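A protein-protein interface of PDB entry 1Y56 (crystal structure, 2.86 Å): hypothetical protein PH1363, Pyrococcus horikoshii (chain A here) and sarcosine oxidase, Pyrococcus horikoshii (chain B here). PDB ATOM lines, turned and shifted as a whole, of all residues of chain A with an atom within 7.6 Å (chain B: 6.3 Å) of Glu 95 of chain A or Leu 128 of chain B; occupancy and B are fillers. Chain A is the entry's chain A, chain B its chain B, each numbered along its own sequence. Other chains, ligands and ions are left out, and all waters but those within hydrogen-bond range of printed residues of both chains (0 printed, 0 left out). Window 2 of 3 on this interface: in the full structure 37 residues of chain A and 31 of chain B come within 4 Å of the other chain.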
ATOM      1  N   GLY A  68       5.773 -12.176  -9.167  1.00  0.00           N
ATOM      2  CA  GLY A  68       7.152 -12.606  -8.958  1.00  0.00           C
ATOM      3  C   GLY A  68       7.757 -12.078  -7.663  1.00  0.00           C
ATOM      4  O   GLY A  68       8.833 -12.520  -7.252  1.00  0.00           O
ATOM      5  N   VAL A  69       7.077 -11.127  -7.023  1.00  0.00           N
ATOM      6  CA  VAL A  69       7.483 -10.662  -5.698  1.00  0.00           C
ATOM      7  C   VAL A  69       6.881 -11.562  -4.605  1.00  0.00           C
ATOM      8  O   VAL A  69       5.668 -11.564  -4.368  1.00  0.00           O
ATOM      9  CB  VAL A  69       7.093  -9.196  -5.456  1.00  0.00           C
ATOM     10  CG1 VAL A  69       7.695  -8.700  -4.149  1.00  0.00           C
ATOM     11  CG2 VAL A  69       7.530  -8.319  -6.622  1.00  0.00           C
ATOM     12  N   LYS A  70       7.742 -12.334  -3.954  1.00  0.00           N
ATOM     13  CA  LYS A  70       7.307 -13.300  -2.960  1.00  0.00           C
ATOM     14  C   LYS A  70       6.961 -12.606  -1.641  1.00  0.00           C
ATOM     15  O   LYS A  70       7.403 -11.491  -1.377  1.00  0.00           O
ATOM     16  CB  LYS A  70       8.394 -14.356  -2.729  1.00  0.00           C
ATOM     17  CG  LYS A  70       8.917 -15.012  -3.986  1.00  0.00           C
ATOM     18  CD  LYS A  70       9.356 -16.432  -3.712  1.00  0.00           C
ATOM     19  CE  LYS A  70      10.831 -16.517  -3.400  1.00  0.00           C
ATOM     20  NZ  LYS A  70      11.595 -16.668  -4.657  1.00  0.00           N
ATOM     21  N   PHE A  93      10.391 -15.259   1.103  1.00  0.00           N
ATOM     22  CA  PHE A  93      10.513 -13.813   1.052  1.00  0.00           C
ATOM     23  C   PHE A  93      11.111 -13.343  -0.265  1.00  0.00           C
ATOM     24  O   PHE A  93      11.740 -14.115  -1.000  1.00  0.00           O
ATOM     25  CB  PHE A  93      11.355 -13.310   2.224  1.00  0.00           C
ATOM     26  CG  PHE A  93      12.772 -13.817   2.220  1.00  0.00           C
ATOM     27  CD1 PHE A  93      13.838 -12.923   2.133  1.00  0.00           C
ATOM     28  CD2 PHE A  93      13.044 -15.187   2.304  1.00  0.00           C
ATOM     29  CE1 PHE A  93      15.158 -13.382   2.131  1.00  0.00           C
ATOM     30  CE2 PHE A  93      14.362 -15.663   2.295  1.00  0.00           C
ATOM     31  CZ  PHE A  93      15.422 -14.759   2.210  1.00  0.00           C
ATOM     32  N   HIS A  94      10.880 -12.067  -0.549  1.00  0.00           N
ATOM     33  CA  HIS A  94      11.490 -11.380  -1.667  1.00  0.00           C
ATOM     34  C   HIS A  94      12.882 -10.918  -1.268  1.00  0.00           C
ATOM     35  O   HIS A  94      13.145 -10.682  -0.092  1.00  0.00           O
ATOM     36  CB  HIS A  94      10.630 -10.180  -2.057  1.00  0.00           C
ATOM     37  CG  HIS A  94      11.045  -9.536  -3.341  1.00  0.00           C
ATOM     38  ND1 HIS A  94      11.302 -10.262  -4.488  1.00  0.00           N
ATOM     39  CD2 HIS A  94      11.249  -8.236  -3.663  1.00  0.00           C
ATOM     40  CE1 HIS A  94      11.647  -9.437  -5.459  1.00  0.00           C
ATOM     41  NE2 HIS A  94      11.627  -8.203  -4.984  1.00  0.00           N
ATOM     42  N   GLU A  95      13.761 -10.759  -2.249  1.00  0.00           N
ATOM     43  CA  GLU A  95      15.173 -10.501  -1.980  1.00  0.00           C
ATOM     44  C   GLU A  95      15.695  -9.060  -2.202  1.00  0.00           C
ATOM     45  O   GLU A  95      16.816  -8.765  -1.819  1.00  0.00           O
ATOM     46  CB  GLU A  95      15.999 -11.490  -2.783  1.00  0.00           C
ATOM     47  CG  GLU A  95      17.118 -12.093  -2.010  1.00  0.00           C
ATOM     48  CD  GLU A  95      17.335 -13.545  -2.371  1.00  0.00           C
ATOM     49  OE1 GLU A  95      16.598 -14.403  -1.844  1.00  0.00           O
ATOM     50  OE2 GLU A  95      18.245 -13.834  -3.175  1.00  0.00           O
ATOM     51  N   GLU A  96      14.894  -8.175  -2.797  1.00  0.00           N
ATOM     52  CA  GLU A  96      15.294  -6.779  -3.038  1.00  0.00           C
ATOM     53  C   GLU A  96      14.371  -5.767  -2.333  1.00  0.00           C
ATOM     54  O   GLU A  96      14.309  -4.584  -2.690  1.00  0.00           O
ATOM     55  CB  GLU A  96      15.329  -6.491  -4.540  1.00  0.00           C
ATOM     56  CG  GLU A  96      16.284  -7.367  -5.348  1.00  0.00           C
ATOM     57  CD  GLU A  96      15.739  -8.775  -5.620  1.00  0.00           C
ATOM     58  OE1 GLU A  96      16.535  -9.661  -5.994  1.00  0.00           O
ATOM     59  OE2 GLU A  96      14.523  -9.015  -5.459  1.00  0.00           O
ATOM     60  N   LYS B 123      30.769 -13.323   1.761  1.00  0.00           N
ATOM     61  CA  LYS B 123      29.497 -13.377   1.049  1.00  0.00           C
ATOM     62  C   LYS B 123      29.089 -14.798   0.613  1.00  0.00           C
ATOM     63  O   LYS B 123      27.915 -15.048   0.356  1.00  0.00           O
ATOM     64  CB  LYS B 123      29.518 -12.422  -0.148  1.00  0.00           C
ATOM     65  CG  LYS B 123      28.177 -12.252  -0.867  1.00  0.00           C
ATOM     66  CD  LYS B 123      28.318 -11.308  -2.054  1.00  0.00           C
ATOM     67  CE  LYS B 123      27.107 -11.339  -2.974  1.00  0.00           C
ATOM     68  NZ  LYS B 123      25.878 -10.884  -2.278  1.00  0.00           N
ATOM     69  N   ILE B 125      29.516 -17.710   2.648  1.00  0.00           N
ATOM     70  CA  ILE B 125      28.796 -17.738   3.922  1.00  0.00           C
ATOM     71  C   ILE B 125      27.868 -16.532   3.827  1.00  0.00           C
ATOM     72  O   ILE B 125      28.291 -15.488   3.339  1.00  0.00           O
ATOM     73  CB  ILE B 125      29.759 -17.473   5.098  1.00  0.00           C
ATOM     74  CG1 ILE B 125      31.144 -18.083   4.832  1.00  0.00           C
ATOM     75  CG2 ILE B 125      29.160 -17.980   6.390  1.00  0.00           C
ATOM     76  CD1 ILE B 125      32.223 -17.662   5.813  1.00  0.00           C
ATOM     77  N   VAL B 126      26.618 -16.627   4.259  1.00  0.00           N
ATOM     78  CA  VAL B 126      25.720 -15.434   4.185  1.00  0.00           C
ATOM     79  C   VAL B 126      25.638 -14.755   2.791  1.00  0.00           C
ATOM     80  O   VAL B 126      26.118 -13.637   2.607  1.00  0.00           O
ATOM     81  CB  VAL B 126      26.069 -14.326   5.243  1.00  0.00           C
ATOM     82  CG1 VAL B 126      24.843 -13.481   5.537  1.00  0.00           C
ATOM     83  CG2 VAL B 126      26.591 -14.927   6.529  1.00  0.00           C
ATOM     84  N   PRO B 127      25.018 -15.431   1.809  1.00  0.00           N
ATOM     85  CA  PRO B 127      24.904 -14.844   0.472  1.00  0.00           C
ATOM     86  C   PRO B 127      24.244 -13.466   0.398  1.00  0.00           C
ATOM     87  O   PRO B 127      24.558 -12.708  -0.514  1.00  0.00           O
ATOM     88  CB  PRO B 127      24.074 -15.876  -0.292  1.00  0.00           C
ATOM     89  CG  PRO B 127      24.301 -17.151   0.433  1.00  0.00           C
ATOM     90  CD  PRO B 127      24.411 -16.777   1.866  1.00  0.00           C
ATOM     91  N   LEU B 128      23.361 -13.138   1.345  1.00  0.00           N
ATOM     92  CA  LEU B 128      22.604 -11.858   1.314  1.00  0.00           C
ATOM     93  C   LEU B 128      23.339 -10.629   1.868  1.00  0.00           C
ATOM     94  O   LEU B 128      22.802  -9.512   1.846  1.00  0.00           O
ATOM     95  CB  LEU B 128      21.261 -11.995   2.029  1.00  0.00           C
ATOM     96  CG  LEU B 128      20.173 -12.835   1.374  1.00  0.00           C
ATOM     97  CD1 LEU B 128      18.947 -12.836   2.246  1.00  0.00           C
ATOM     98  CD2 LEU B 128      19.850 -12.279   0.024  1.00  0.00           C
ATOM     99  N   LEU B 129      24.552 -10.850   2.373  1.00  0.00           N
ATOM    100  CA  LEU B 129      25.432  -9.784   2.823  1.00  0.00           C
ATOM    101  C   LEU B 129      25.694  -8.771   1.715  1.00  0.00           C
ATOM    102  O   LEU B 129      26.046  -9.161   0.598  1.00  0.00           O
ATOM    103  CB  LEU B 129      26.755 -10.404   3.225  1.00  0.00           C
ATOM    104  CG  LEU B 129      27.391  -9.966   4.529  1.00  0.00           C
ATOM    105  CD1 LEU B 129      26.349  -9.860   5.622  1.00  0.00           C
ATOM    106  CD2 LEU B 129      28.449 -10.996   4.892  1.00  0.00           C
ATOM    107  N   ASP B 130      25.513  -7.480   2.002  1.00  0.00           N
ATOM    108  CA  ASP B 130      25.947  -6.442   1.061  1.00  0.00           C
ATOM    109  C   ASP B 130      27.440  -6.265   1.218  1.00  0.00           C
ATOM    110  O   ASP B 130      27.919  -5.906   2.300  1.00  0.00           O
ATOM    111  CB  ASP B 130      25.244  -5.109   1.295  1.00  0.00           C
ATOM    112  CG  ASP B 130      25.736  -4.002   0.354  1.00  0.00           C
ATOM    113  OD1 ASP B 130      25.234  -2.864   0.469  1.00  0.00           O
ATOM    114  OD2 ASP B 130      26.620  -4.253  -0.497  1.00  0.00           O
ATOM    115  N   THR B 237      19.258 -19.206   6.005  1.00  0.00           N
ATOM    116  CA  THR B 237      19.486 -17.964   5.278  1.00  0.00           C
ATOM    117  C   THR B 237      20.621 -17.166   5.922  1.00  0.00           C
ATOM    118  O   THR B 237      21.517 -16.716   5.218  1.00  0.00           O
ATOM    119  CB  THR B 237      18.198 -17.123   5.159  1.00  0.00           C
ATOM    120  OG1 THR B 237      17.263 -17.812   4.320  1.00  0.00           O
ATOM    121  CG2 THR B 237      18.485 -15.741   4.563  1.00  0.00           C
ATOM    122  N   ILE B 238      20.592 -16.986   7.243  1.00  0.00           N
ATOM    123  CA  ILE B 238      21.716 -16.350   7.943  1.00  0.00           C
ATOM    124  C   ILE B 238      22.239 -17.278   9.026  1.00  0.00           C
ATOM    125  O   ILE B 238      21.661 -17.361  10.107  1.00  0.00           O
ATOM    126  CB  ILE B 238      21.366 -14.985   8.592  1.00  0.00           C
ATOM    127  CG1 ILE B 238      20.534 -14.106   7.653  1.00  0.00           C
ATOM    128  CG2 ILE B 238      22.645 -14.273   9.029  1.00  0.00           C
ATOM    129  CD1 ILE B 238      20.039 -12.822   8.317  1.00  0.00           C
ATOM    130  N   ILE B 291      23.555  -3.537   6.571  1.00  0.00           N
ATOM    131  CA  ILE B 291      24.426  -4.721   6.568  1.00  0.00           C
ATOM    132  C   ILE B 291      23.866  -5.846   5.674  1.00  0.00           C
ATOM    133  O   ILE B 291      24.604  -6.398   4.860  1.00  0.00           O
ATOM    134  CB  ILE B 291      24.961  -5.182   8.010  1.00  0.00           C
ATOM    135  CG1 ILE B 291      24.452  -6.547   8.398  1.00  0.00           C
ATOM    136  CG2 ILE B 291      24.745  -4.167   9.127  1.00  0.00           C
ATOM    137  CD1 ILE B 291      25.371  -7.601   7.924  1.00  0.00           C
ATOM    138  N   ILE B 292      22.585  -6.183   5.814  1.00  0.00           N
ATOM    139  CA  ILE B 292      21.941  -7.035   4.817  1.00  0.00           C
ATOM    140  C   ILE B 292      20.641  -6.361   4.359  1.00  0.00           C
ATOM    141  O   ILE B 292      19.665  -6.343   5.092  1.00  0.00           O
ATOM    142  CB  ILE B 292      21.786  -8.582   5.228  1.00  0.00           C
ATOM    143  CG1 ILE B 292      20.347  -8.999   5.451  1.00  0.00           C
ATOM    144  CG2 ILE B 292      22.614  -9.018   6.434  1.00  0.00           C
ATOM    145  CD1 ILE B 292      19.674  -9.523   4.202  1.00  0.00           C
ATOM    146  N   PRO B 293      20.657  -5.736   3.164  1.00  0.00           N
ATOM    147  CA  PRO B 293      19.552  -5.026   2.503  1.00  0.00           C
ATOM    148  C   PRO B 293      18.215  -5.756   2.340  1.00  0.00           C
ATOM    149  O   PRO B 293      17.174  -5.092   2.309  1.00  0.00           O
ATOM    150  CB  PRO B 293      20.127  -4.714   1.121  1.00  0.00           C
ATOM    151  CG  PRO B 293      21.548  -4.534   1.382  1.00  0.00           C
ATOM    152  CD  PRO B 293      21.884  -5.627   2.358  1.00  0.00           C
ATOM    153  N   ALA B 294      18.229  -7.084   2.214  1.00  0.00           N
ATOM    154  CA  ALA B 294      16.984  -7.849   2.076  1.00  0.00           C
ATOM    155  C   ALA B 294      16.054  -7.665   3.280  1.00  0.00           C
ATOM    156  O   ALA B 294      14.827  -7.635   3.131  1.00  0.00           O
ATOM    157  CB  ALA B 294      17.282  -9.329   1.841  1.00  0.00           C
ATOM    158  N   LEU B 295      16.652  -7.526   4.464  1.00  0.00           N
ATOM    159  CA  LEU B 295      15.920  -7.214   5.700  1.00  0.00           C
ATOM    160  C   LEU B 295      14.887  -6.088   5.561  1.00  0.00           C
ATOM    161  O   LEU B 295      13.905  -6.064   6.294  1.00  0.00           O
ATOM    162  CB  LEU B 295      16.894  -6.915   6.845  1.00  0.00           C
ATOM    163  CG  LEU B 295      17.386  -8.022   7.802  1.00  0.00           C
ATOM    164  CD1 LEU B 295      17.376  -9.440   7.236  1.00  0.00           C
ATOM    165  CD2 LEU B 295      18.773  -7.691   8.356  1.00  0.00           C
ATOM    166  N   ASN B 297      12.552  -5.788   3.378  1.00  0.00           N
ATOM    167  CA  ASN B 297      11.239  -6.359   3.042  1.00  0.00           C
ATOM    168  C   ASN B 297      10.642  -7.217   4.170  1.00  0.00           C
ATOM    169  O   ASN B 297       9.535  -7.747   4.047  1.00  0.00           O
ATOM    170  CB  ASN B 297      11.304  -7.187   1.745  1.00  0.00           C
ATOM    171  CG  ASN B 297      12.185  -6.550   0.660  1.00  0.00           C
ATOM    172  OD1 ASN B 297      12.280  -5.317   0.533  1.00  0.00           O
ATOM    173  ND2 ASN B 297      12.833  -7.404  -0.133  1.00  0.00           N
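The side-chain amide nitrogen (ND2) of Asn 297 of chain B sits at hydrogen-bond distance from the backbone carbonyl oxygen (O) of His 94 of chain A. The backbone NH (N) of Glu 96 of chain A sits close to the side-chain amide nitrogen (ND2) of Asn 297 of chain B (3.5 Å).
OE2 of Glu 96 of chain A sits close to NE2 of His 94 of chain A, at 3.0 Å.
Leu 128 of chain B touches Phe 93 of chain A. CG2 of Thr 237 of chain B touches CZ of Phe 93 of chain A, at 3.99 Å. CD2 of Leu 128 of chain B touches CG of Glu 95 of chain A, at 3.4 Å. Ala 294 of chain B touches Glu 95 of chain A (CB to O, 3.7 Å). Glu 95 of chain A touches Asn 297 of chain B (C to ND2, 3.9 Å).
Of chain B, only Leu 128 (3.4 Å), Ala 294 (3.7 Å) and Asn 297 (3.9 Å) come within 4 Å of Glu 95 of chain A. Of chain A, only Phe 93 (3.8 Å) and Glu 95 (3.4 Å) come within 4 Å of Leu 128 of chain B. Of the printed residues of chain A, Ala 294 of chain B touches Glu 95. Of the printed residues of chain B, Phe 93 of chain A touches Leu 128 and Thr 237. Printed residues of chain A within 4 Å of Asn 297 of chain B: His 94 (3.3 Å), Glu 95 (3.9 Å) and Glu 96 (3.1 Å). The nearest residue of chain B that does not touch Glu 95 of chain A is Pro 293 of chain B (5.3 Å).
Hydrophobic or aromatic side chains of chain A within 4 Å of the printed part of chain B: Phe 93 and His 94. Along chain A the printed residues that touch a printed residue of chain B span positions 93 to 96. Hydrophobic or aromatic side chains of chain B within 4 Å of the printed part of chain A: Leu 128 and Ala 294.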
